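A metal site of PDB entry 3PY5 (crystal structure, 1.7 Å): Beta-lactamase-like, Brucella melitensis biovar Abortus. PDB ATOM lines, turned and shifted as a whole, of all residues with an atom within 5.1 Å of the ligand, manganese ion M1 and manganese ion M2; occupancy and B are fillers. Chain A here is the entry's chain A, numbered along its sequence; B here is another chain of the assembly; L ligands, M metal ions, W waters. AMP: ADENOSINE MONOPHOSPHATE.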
ATOM      1  N   SER A  20      16.032 -22.044  28.174  1.00  0.00           N
ATOM      2  CA  SER A  20      17.274 -22.248  27.413  1.00  0.00           C
ATOM      3  C   SER A  20      18.428 -21.228  27.632  1.00  0.00           C
ATOM      4  O   SER A  20      19.558 -21.618  27.555  1.00  0.00           O
ATOM      5  CB  SER A  20      17.021 -22.439  25.927  1.00  0.00           C
ATOM      6  OG  SER A  20      16.478 -21.283  25.347  1.00  0.00           O
ATOM      7  N   HIS A  88      15.455 -34.774  24.037  1.00  0.00           N
ATOM      8  CA  HIS A  88      15.350 -34.157  22.715  1.00  0.00           C
ATOM      9  C   HIS A  88      16.663 -33.378  22.430  1.00  0.00           C
ATOM     10  O   HIS A  88      17.382 -33.038  23.383  1.00  0.00           O
ATOM     11  CB  HIS A  88      14.131 -33.250  22.524  1.00  0.00           C
ATOM     12  CG  HIS A  88      14.204 -31.920  23.238  1.00  0.00           C
ATOM     13  ND1 HIS A  88      14.343 -31.813  24.612  1.00  0.00           N
ATOM     14  CD2 HIS A  88      14.062 -30.653  22.778  1.00  0.00           C
ATOM     15  CE1 HIS A  88      14.287 -30.545  24.958  1.00  0.00           C
ATOM     16  NE2 HIS A  88      14.133 -29.813  23.872  1.00  0.00           N
ATOM     17  N   PRO A  89      16.976 -33.153  21.150  1.00  0.00           N
ATOM     18  CA  PRO A  89      18.276 -32.557  20.810  1.00  0.00           C
ATOM     19  C   PRO A  89      18.266 -31.042  20.622  1.00  0.00           C
ATOM     20  O   PRO A  89      18.426 -30.552  19.491  1.00  0.00           O
ATOM     21  CB  PRO A  89      18.592 -33.200  19.468  1.00  0.00           C
ATOM     22  CG  PRO A  89      17.240 -33.298  18.792  1.00  0.00           C
ATOM     23  CD  PRO A  89      16.281 -33.671  19.944  1.00  0.00           C
ATOM     24  N   HIS A  90      17.996 -30.329  21.686  1.00  0.00           N
ATOM     25  CA  HIS A  90      18.129 -28.892  21.706  1.00  0.00           C
ATOM     26  C   HIS A  90      19.356 -28.556  22.574  1.00  0.00           C
ATOM     27  O   HIS A  90      19.687 -29.261  23.532  1.00  0.00           O
ATOM     28  CB  HIS A  90      16.860 -28.220  22.226  1.00  0.00           C
ATOM     29  CG  HIS A  90      15.775 -28.091  21.198  1.00  0.00           C
ATOM     30  ND1 HIS A  90      14.476 -27.745  21.517  1.00  0.00           N
ATOM     31  CD2 HIS A  90      15.783 -28.291  19.844  1.00  0.00           C
ATOM     32  CE1 HIS A  90      13.756 -27.679  20.411  1.00  0.00           C
ATOM     33  NE2 HIS A  90      14.520 -28.013  19.390  1.00  0.00           N
ATOM     34  N   ALA A  91      20.056 -27.503  22.163  1.00  0.00           N
ATOM     35  CA  ALA A  91      21.300 -27.014  22.785  1.00  0.00           C
ATOM     36  C   ALA A  91      21.345 -27.129  24.328  1.00  0.00           C
ATOM     37  O   ALA A  91      22.309 -27.653  24.938  1.00  0.00           O
ATOM     38  CB  ALA A  91      21.491 -25.515  22.379  1.00  0.00           C
ATOM     39  N   ASP A  92      20.308 -26.615  24.944  1.00  0.00           N
ATOM     40  CA  ASP A  92      20.238 -26.528  26.390  1.00  0.00           C
ATOM     41  C   ASP A  92      20.139 -27.880  27.088  1.00  0.00           C
ATOM     42  O   ASP A  92      20.206 -27.908  28.305  1.00  0.00           O
ATOM     43  CB  ASP A  92      19.137 -25.562  26.860  1.00  0.00           C
ATOM     44  CG  ASP A  92      17.760 -25.843  26.258  1.00  0.00           C
ATOM     45  OD1 ASP A  92      17.684 -26.082  25.030  1.00  0.00           O
ATOM     46  OD2 ASP A  92      16.790 -25.723  27.030  1.00  0.00           O
ATOM     47  N   HIS A  93      19.958 -28.963  26.313  1.00  0.00           N
ATOM     48  CA  HIS A  93      19.837 -30.319  26.798  1.00  0.00           C
ATOM     49  C   HIS A  93      20.962 -31.261  26.382  1.00  0.00           C
ATOM     50  O   HIS A  93      21.082 -32.374  26.921  1.00  0.00           O
ATOM     51  CB  HIS A  93      18.435 -30.877  26.362  1.00  0.00           C
ATOM     52  CG  HIS A  93      17.291 -30.018  26.834  1.00  0.00           C
ATOM     53  ND1 HIS A  93      16.525 -30.333  27.944  1.00  0.00           N
ATOM     54  CD2 HIS A  93      16.770 -28.888  26.317  1.00  0.00           C
ATOM     55  CE1 HIS A  93      15.594 -29.405  28.087  1.00  0.00           C
ATOM     56  NE2 HIS A  93      15.712 -28.515  27.110  1.00  0.00           N
ATOM     57  N   ILE A  94      21.856 -30.808  25.502  1.00  0.00           N
ATOM     58  CA  ILE A  94      22.873 -31.694  24.993  1.00  0.00           C
ATOM     59  C   ILE A  94      24.308 -31.131  24.930  1.00  0.00           C
ATOM     60  O   ILE A  94      25.239 -31.908  24.812  1.00  0.00           O
ATOM     61  CB  ILE A  94      22.475 -32.241  23.591  1.00  0.00           C
ATOM     62  CG1 ILE A  94      22.255 -31.098  22.559  1.00  0.00           C
ATOM     63  CG2 ILE A  94      21.270 -33.236  23.710  1.00  0.00           C
ATOM     64  CD1 ILE A  94      22.183 -31.580  21.084  1.00  0.00           C
ATOM     65  N   HIS A  95      24.500 -29.826  25.001  1.00  0.00           N
ATOM     66  CA  HIS A  95      25.801 -29.249  24.711  1.00  0.00           C
ATOM     67  C   HIS A  95      26.869 -29.411  25.818  1.00  0.00           C
ATOM     68  O   HIS A  95      28.006 -28.987  25.640  1.00  0.00           O
ATOM     69  CB  HIS A  95      25.654 -27.785  24.270  1.00  0.00           C
ATOM     70  CG  HIS A  95      25.121 -27.627  22.882  1.00  0.00           C
ATOM     71  ND1 HIS A  95      24.852 -26.392  22.333  1.00  0.00           N
ATOM     72  CD2 HIS A  95      24.808 -28.538  21.924  1.00  0.00           C
ATOM     73  CE1 HIS A  95      24.388 -26.550  21.102  1.00  0.00           C
ATOM     74  NE2 HIS A  95      24.357 -27.842  20.824  1.00  0.00           N
ATOM     75  N   HIS A 172       6.476 -30.801  21.224  1.00  0.00           N
ATOM     76  CA  HIS A 172       7.339 -29.695  21.615  1.00  0.00           C
ATOM     77  C   HIS A 172       7.470 -28.741  20.438  1.00  0.00           C
ATOM     78  O   HIS A 172       8.458 -28.726  19.720  1.00  0.00           O
ATOM     79  CB  HIS A 172       8.697 -30.266  22.031  1.00  0.00           C
ATOM     80  CG  HIS A 172       9.680 -29.232  22.478  1.00  0.00           C
ATOM     81  ND1 HIS A 172       9.307 -28.061  23.104  1.00  0.00           N
ATOM     82  CD2 HIS A 172      11.030 -29.206  22.408  1.00  0.00           C
ATOM     83  CE1 HIS A 172      10.389 -27.357  23.409  1.00  0.00           C
ATOM     84  NE2 HIS A 172      11.444 -28.035  23.008  1.00  0.00           N
ATOM     85  N   ASP A 190       9.906 -29.361  28.215  1.00  0.00           N
ATOM     86  CA  ASP A 190       9.901 -29.066  26.770  1.00  0.00           C
ATOM     87  C   ASP A 190       8.713 -29.722  26.073  1.00  0.00           C
ATOM     88  O   ASP A 190       8.843 -30.537  25.143  1.00  0.00           O
ATOM     89  CB  ASP A 190      11.251 -29.429  26.133  1.00  0.00           C
ATOM     90  CG  ASP A 190      12.390 -28.576  26.657  1.00  0.00           C
ATOM     91  OD1 ASP A 190      12.848 -28.792  27.791  1.00  0.00           O
ATOM     92  OD2 ASP A 190      12.823 -27.687  25.935  1.00  0.00           O
ATOM     93  N   HIS A 218       3.527 -19.537  24.209  1.00  0.00           N
ATOM     94  CA  HIS A 218       4.764 -19.793  23.491  1.00  0.00           C
ATOM     95  C   HIS A 218       4.517 -21.002  22.639  1.00  0.00           C
ATOM     96  O   HIS A 218       3.822 -21.920  23.060  1.00  0.00           O
ATOM     97  CB  HIS A 218       5.915 -20.112  24.430  1.00  0.00           C
ATOM     98  CG  HIS A 218       7.266 -20.117  23.757  1.00  0.00           C
ATOM     99  ND1 HIS A 218       7.743 -21.209  23.074  1.00  0.00           N
ATOM    100  CD2 HIS A 218       8.233 -19.180  23.694  1.00  0.00           C
ATOM    101  CE1 HIS A 218       8.956 -20.928  22.605  1.00  0.00           C
ATOM    102  NE2 HIS A 218       9.273 -19.702  22.984  1.00  0.00           N
ATOM    103  N   SER A 220       6.308 -23.559  21.882  1.00  0.00           N
ATOM    104  CA  SER A 220       7.043 -24.774  22.208  1.00  0.00           C
ATOM    105  C   SER A 220       6.899 -25.240  23.653  1.00  0.00           C
ATOM    106  O   SER A 220       7.466 -26.307  24.045  1.00  0.00           O
ATOM    107  CB  SER A 220       8.532 -24.550  21.954  1.00  0.00           C
ATOM    108  OG  SER A 220       8.759 -24.195  20.604  1.00  0.00           O
ATOM    109  N   HIS A 221       6.251 -24.431  24.489  1.00  0.00           N
ATOM    110  CA  HIS A 221       6.121 -24.759  25.899  1.00  0.00           C
ATOM    111  C   HIS A 221       4.816 -24.333  26.444  1.00  0.00           C
ATOM    112  O   HIS A 221       4.264 -23.305  26.024  1.00  0.00           O
ATOM    113  CB  HIS A 221       7.160 -24.033  26.726  1.00  0.00           C
ATOM    114  CG  HIS A 221       8.575 -24.254  26.277  1.00  0.00           C
ATOM    115  ND1 HIS A 221       9.359 -25.260  26.797  1.00  0.00           N
ATOM    116  CD2 HIS A 221       9.354 -23.574  25.398  1.00  0.00           C
ATOM    117  CE1 HIS A 221      10.551 -25.207  26.238  1.00  0.00           C
ATOM    118  NE2 HIS A 221      10.572 -24.204  25.370  1.00  0.00           N
ATOM    119  N   HIS A 243      11.773 -25.628  33.773  1.00  0.00           N
ATOM    120  CA  HIS A 243      12.030 -24.928  32.499  1.00  0.00           C
ATOM    121  C   HIS A 243      11.429 -23.559  32.504  1.00  0.00           C
ATOM    122  O   HIS A 243      10.904 -23.117  31.487  1.00  0.00           O
ATOM    123  CB  HIS A 243      11.571 -25.743  31.283  1.00  0.00           C
ATOM    124  CG  HIS A 243      12.384 -25.538  30.064  1.00  0.00           C
ATOM    125  ND1 HIS A 243      12.278 -24.396  29.297  1.00  0.00           N
ATOM    126  CD2 HIS A 243      13.304 -26.318  29.441  1.00  0.00           C
ATOM    127  CE1 HIS A 243      13.065 -24.508  28.239  1.00  0.00           C
ATOM    128  NE2 HIS A 243      13.730 -25.642  28.330  1.00  0.00           N
ATOM    129  N   ASP B  98      25.840 -21.586  21.664  1.00  0.00           N
ATOM    130  CA  ASP B  98      24.417 -21.254  21.562  1.00  0.00           C
ATOM    131  C   ASP B  98      24.127 -20.027  22.387  1.00  0.00           C
ATOM    132  O   ASP B  98      23.184 -19.269  22.092  1.00  0.00           O
ATOM    133  CB  ASP B  98      23.537 -22.398  22.039  1.00  0.00           C
ATOM    134  CG  ASP B  98      22.098 -22.138  21.772  1.00  0.00           C
ATOM    135  OD1 ASP B  98      21.654 -22.356  20.650  1.00  0.00           O
ATOM    136  OD2 ASP B  98      21.418 -21.689  22.701  1.00  0.00           O
ATOM    137  N   ARG B 101      23.154 -16.297  21.515  1.00  0.00           N
ATOM    138  CA  ARG B 101      21.841 -15.882  21.008  1.00  0.00           C
ATOM    139  C   ARG B 101      21.314 -14.608  21.652  1.00  0.00           C
ATOM    140  O   ARG B 101      20.765 -13.760  20.947  1.00  0.00           O
ATOM    141  CB  ARG B 101      20.828 -17.016  21.249  1.00  0.00           C
ATOM    142  CG  ARG B 101      19.430 -16.776  20.708  1.00  0.00           C
ATOM    143  CD  ARG B 101      18.625 -18.048  21.007  1.00  0.00           C
ATOM    144  NE  ARG B 101      19.333 -19.169  20.390  1.00  0.00           N
ATOM    145  CZ  ARG B 101      19.261 -19.470  19.091  1.00  0.00           C
ATOM    146  NH1 ARG B 101      18.479 -18.759  18.290  1.00  0.00           N
ATOM    147  NH2 ARG B 101      19.971 -20.485  18.582  1.00  0.00           N
ATOM    148  N   TYR B 129      22.826 -25.099  12.672  1.00  0.00           N
ATOM    149  CA  TYR B 129      21.645 -24.283  12.925  1.00  0.00           C
ATOM    150  C   TYR B 129      21.955 -22.834  13.332  1.00  0.00           C
ATOM    151  O   TYR B 129      21.095 -21.946  13.262  1.00  0.00           O
ATOM    152  CB  TYR B 129      20.753 -24.953  13.978  1.00  0.00           C
ATOM    153  CG  TYR B 129      21.298 -24.794  15.368  1.00  0.00           C
ATOM    154  CD1 TYR B 129      22.299 -25.625  15.840  1.00  0.00           C
ATOM    155  CD2 TYR B 129      20.797 -23.827  16.210  1.00  0.00           C
ATOM    156  CE1 TYR B 129      22.792 -25.457  17.110  1.00  0.00           C
ATOM    157  CE2 TYR B 129      21.290 -23.663  17.470  1.00  0.00           C
ATOM    158  CZ  TYR B 129      22.280 -24.478  17.937  1.00  0.00           C
ATOM    159  OH  TYR B 129      22.765 -24.241  19.201  1.00  0.00           O
ATOM    160  N   PRO B 134      17.822 -25.214   9.490  1.00  0.00           N
ATOM    161  CA  PRO B 134      17.650 -26.517   8.867  1.00  0.00           C
ATOM    162  C   PRO B 134      16.224 -26.855   8.516  1.00  0.00           C
ATOM    163  O   PRO B 134      15.265 -26.222   9.027  1.00  0.00           O
ATOM    164  CB  PRO B 134      18.117 -27.493   9.939  1.00  0.00           C
ATOM    165  CG  PRO B 134      17.804 -26.851  11.205  1.00  0.00           C
ATOM    166  CD  PRO B 134      18.006 -25.337  10.955  1.00  0.00           C
ATOM    167  N   SER B 137      12.631 -26.479  10.844  1.00  0.00           N
ATOM    168  CA  SER B 137      12.868 -25.525  11.960  1.00  0.00           C
ATOM    169  C   SER B 137      12.401 -24.130  11.604  1.00  0.00           C
ATOM    170  O   SER B 137      12.369 -23.735  10.444  1.00  0.00           O
ATOM    171  CB  SER B 137      14.365 -25.483  12.308  1.00  0.00           C
ATOM    172  OG  SER B 137      14.637 -24.513  13.330  1.00  0.00           O
ATOM    173  N   TYR B 139      13.838 -21.578  13.686  1.00  0.00           N
ATOM    174  CA  TYR B 139      14.831 -20.747  14.365  1.00  0.00           C
ATOM    175  C   TYR B 139      15.716 -20.037  13.329  1.00  0.00           C
ATOM    176  O   TYR B 139      16.386 -20.694  12.516  1.00  0.00           O
ATOM    177  CB  TYR B 139      15.688 -21.598  15.337  1.00  0.00           C
ATOM    178  CG  TYR B 139      14.966 -21.990  16.606  1.00  0.00           C
ATOM    179  CD1 TYR B 139      14.864 -21.117  17.672  1.00  0.00           C
ATOM    180  CD2 TYR B 139      14.394 -23.240  16.756  1.00  0.00           C
ATOM    181  CE1 TYR B 139      14.200 -21.457  18.831  1.00  0.00           C
ATOM    182  CE2 TYR B 139      13.731 -23.610  17.937  1.00  0.00           C
ATOM    183  CZ  TYR B 139      13.636 -22.709  18.960  1.00  0.00           C
ATOM    184  OH  TYR B 139      13.006 -23.018  20.137  1.00  0.00           O
HETATM  185  P   AMP L   1      13.694 -24.465  24.160  1.00  0.00           P
HETATM  186  O1P AMP L   1      13.016 -25.587  23.336  1.00  0.00           O
HETATM  187  O2P AMP L   1      12.932 -23.141  24.180  1.00  0.00           O
HETATM  188  O3P AMP L   1      14.027 -24.782  25.610  1.00  0.00           O
HETATM  189  O5' AMP L   1      15.106 -24.008  23.504  1.00  0.00           O
HETATM  190  C5' AMP L   1      15.568 -24.243  22.186  1.00  0.00           C
HETATM  191  C4' AMP L   1      17.091 -24.284  22.329  1.00  0.00           C
HETATM  192  O4' AMP L   1      17.628 -25.074  21.274  1.00  0.00           O
HETATM  193  C3' AMP L   1      17.783 -22.926  22.238  1.00  0.00           C
HETATM  194  O3' AMP L   1      19.024 -23.057  22.925  1.00  0.00           O
HETATM  195  C2' AMP L   1      18.060 -22.814  20.757  1.00  0.00           C
HETATM  196  O2' AMP L   1      19.083 -21.862  20.458  1.00  0.00           O
HETATM  197  C1' AMP L   1      18.457 -24.241  20.471  1.00  0.00           C
HETATM  198  N9  AMP L   1      18.294 -24.727  19.088  1.00  0.00           N
HETATM  199  C8  AMP L   1      17.593 -24.147  18.088  1.00  0.00           C
HETATM  200  N7  AMP L   1      17.678 -24.897  16.973  1.00  0.00           N
HETATM  201  C5  AMP L   1      18.458 -25.963  17.269  1.00  0.00           C
HETATM  202  C6  AMP L   1      18.971 -27.109  16.509  1.00  0.00           C
HETATM  203  N6  AMP L   1      18.670 -27.330  15.209  1.00  0.00           N
HETATM  204  N1  AMP L   1      19.750 -27.963  17.206  1.00  0.00           N
HETATM  205  C2  AMP L   1      20.082 -27.769  18.515  1.00  0.00           C
HETATM  206  N3  AMP L   1      19.670 -26.735  19.261  1.00  0.00           N
HETATM  207  C4  AMP L   1      18.854 -25.828  18.675  1.00  0.00           C
HETATM  208 MN    MN M   1      13.632 -27.628  23.600  1.00  0.00          MN
HETATM  209 MN    MN M   2      14.719 -26.632  26.624  1.00  0.00          MN
HETATM  210  O   HOH W   1      22.171 -29.168  15.629  1.00  0.00           O
HETATM  211  O   HOH W   2      20.539 -31.195  17.110  1.00  0.00           O
HETATM  212  O   HOH W   3      17.053 -24.634  14.102  1.00  0.00           O
HETATM  213  O   HOH W   4      19.408 -29.169  13.564  1.00  0.00           O
HETATM  214  O   HOH W   5      15.192 -26.869  24.552  1.00  0.00           O
HETATM  215  O   HOH W   6      11.654 -24.933  21.279  1.00  0.00           O
HETATM  216  O   HOH W   7      13.189 -21.327  22.243  1.00  0.00           O
HETATM  217  O   HOH W   8      17.714 -30.457  16.680  1.00  0.00           O
HETATM  218  O   HOH W   9      21.290 -22.935  25.440  1.00  0.00           O
HETATM  219  O   HOH W  10      13.720 -21.650  26.415  1.00  0.00           O
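The guanidinium group (NH2) of Arg 101 of chain B is in hydrogen-bond range of an oxygen (O2') of the ligand.
OD1 of Asp 98 of chain B sits at hydrogen-bond distance from O2' of the ligand (2.6 Å).
O2P of the ligand sits at hydrogen-bond distance from NE2 of His 221.
The backbone NH of Ala 91 lies within hydrogen-bond range of a nitrogen (N3) of the ligand (3.0 Å).
Four residues have an atom within 4 Å of manganese ion M1: His 88, His 90, His 172 and Asp 190.
The nearest printed residue that does not touch manganese ion M1 is His 93 (4.2 Å).
Water W5 bridges the side-chain carboxylate (OD1) of Asp 92 (2.7 Å) and an oxygen (O5') of the ligand (3.0 Å).
Water W6 bridges the side-chain hydroxyl (OH) of Tyr 139 of chain B (2.6 Å) and the side-chain hydroxyl (OG) of Ser 220 (3.1 Å).
Water W7 lies within hydrogen-bond range of O2P of the ligand (2.7 Å) and OH of Tyr 139 of chain B (2.7 Å).
Water W10 lies within hydrogen-bond range of an oxygen (O2P) of the ligand (2.8 Å) and the backbone NH (N) of Ser 20 (2.9 Å).
Water W3 lies within hydrogen-bond range of the side-chain hydroxyl of Ser 137 of chain B (2.5 Å) and a nitrogen (N7) of the ligand (2.9 Å).
Water W9 lies within hydrogen-bond range of OD2 of Asp 98 of chain B (3.0 Å), O of Ser 20 (3.0 Å) and O3' of the ligand (3.4 Å).
Within 4 Å of manganese ion M2: Asp 92, His 93, Asp 190 and His 243.
The nearest printed residue that does not touch manganese ion M2 is His 88 (4.2 Å).
Water W5 binds manganese ion M2 (2.1 Å).
Manganese ion M2 is bound by NE2 of His 93 (2.2 Å).
Manganese ion M2 is bound by NE2 of His 243.
O3P of the ligand binds manganese ion M2 (2.2 Å).
The side-chain carboxylate (OD2) of Asp 190 is bound to manganese ion M2 (2.3 Å).
OD2 of Asp 92 binds manganese ion M2 (2.3 Å).
Manganese ion M2 has six donor atoms within binding distance.
Manganese ion M1 is bound by water W5 (2.0 Å), O1P of the ligand (2.1 Å), ND1 of His 90 (2.3 Å), NE2 of His 88 (2.3 Å), NE2 of His 172 (2.3 Å) and OD2 of Asp 190 (2.5 Å).
Manganese ion M1 has six donor atoms within binding distance.
Residues that only touch the ligand: Ser 20 (3.5 Å), Pro 89 (3.4 Å), Tyr 129 of chain B (3.3 Å) and Tyr 139 of chain B (3.5 Å).
13 residues have an atom within 4 Å of the ligand: Ser 20, Pro 89, His 90, Ala 91, Asp 92, His 172, Asp 190, His 221, His 243, Asp 98 of chain B, Arg 101 of chain B, Tyr 129 of chain B and Tyr 139 of chain B.
The nearest printed residue that does not touch the ligand is Pro 134 of chain B (4.1 Å).
ND1 of His 172 sits at hydrogen-bond distance from O of Ser 220, 2.7 Å away.
OD1 of Asp 98 of chain B lies within salt-bridge range of NH2 of Arg 101 of chain B, 3.3 Å away.
The side-chain hydroxyl (OH) of Tyr 129 of chain B is in hydrogen-bond range of the side-chain carboxylate (OD1) of Asp 98 of chain B, at 2.6 Å.
N of Tyr 139 of chain B is in hydrogen-bond range of OG of Ser 137 of chain B, 3.1 Å away.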
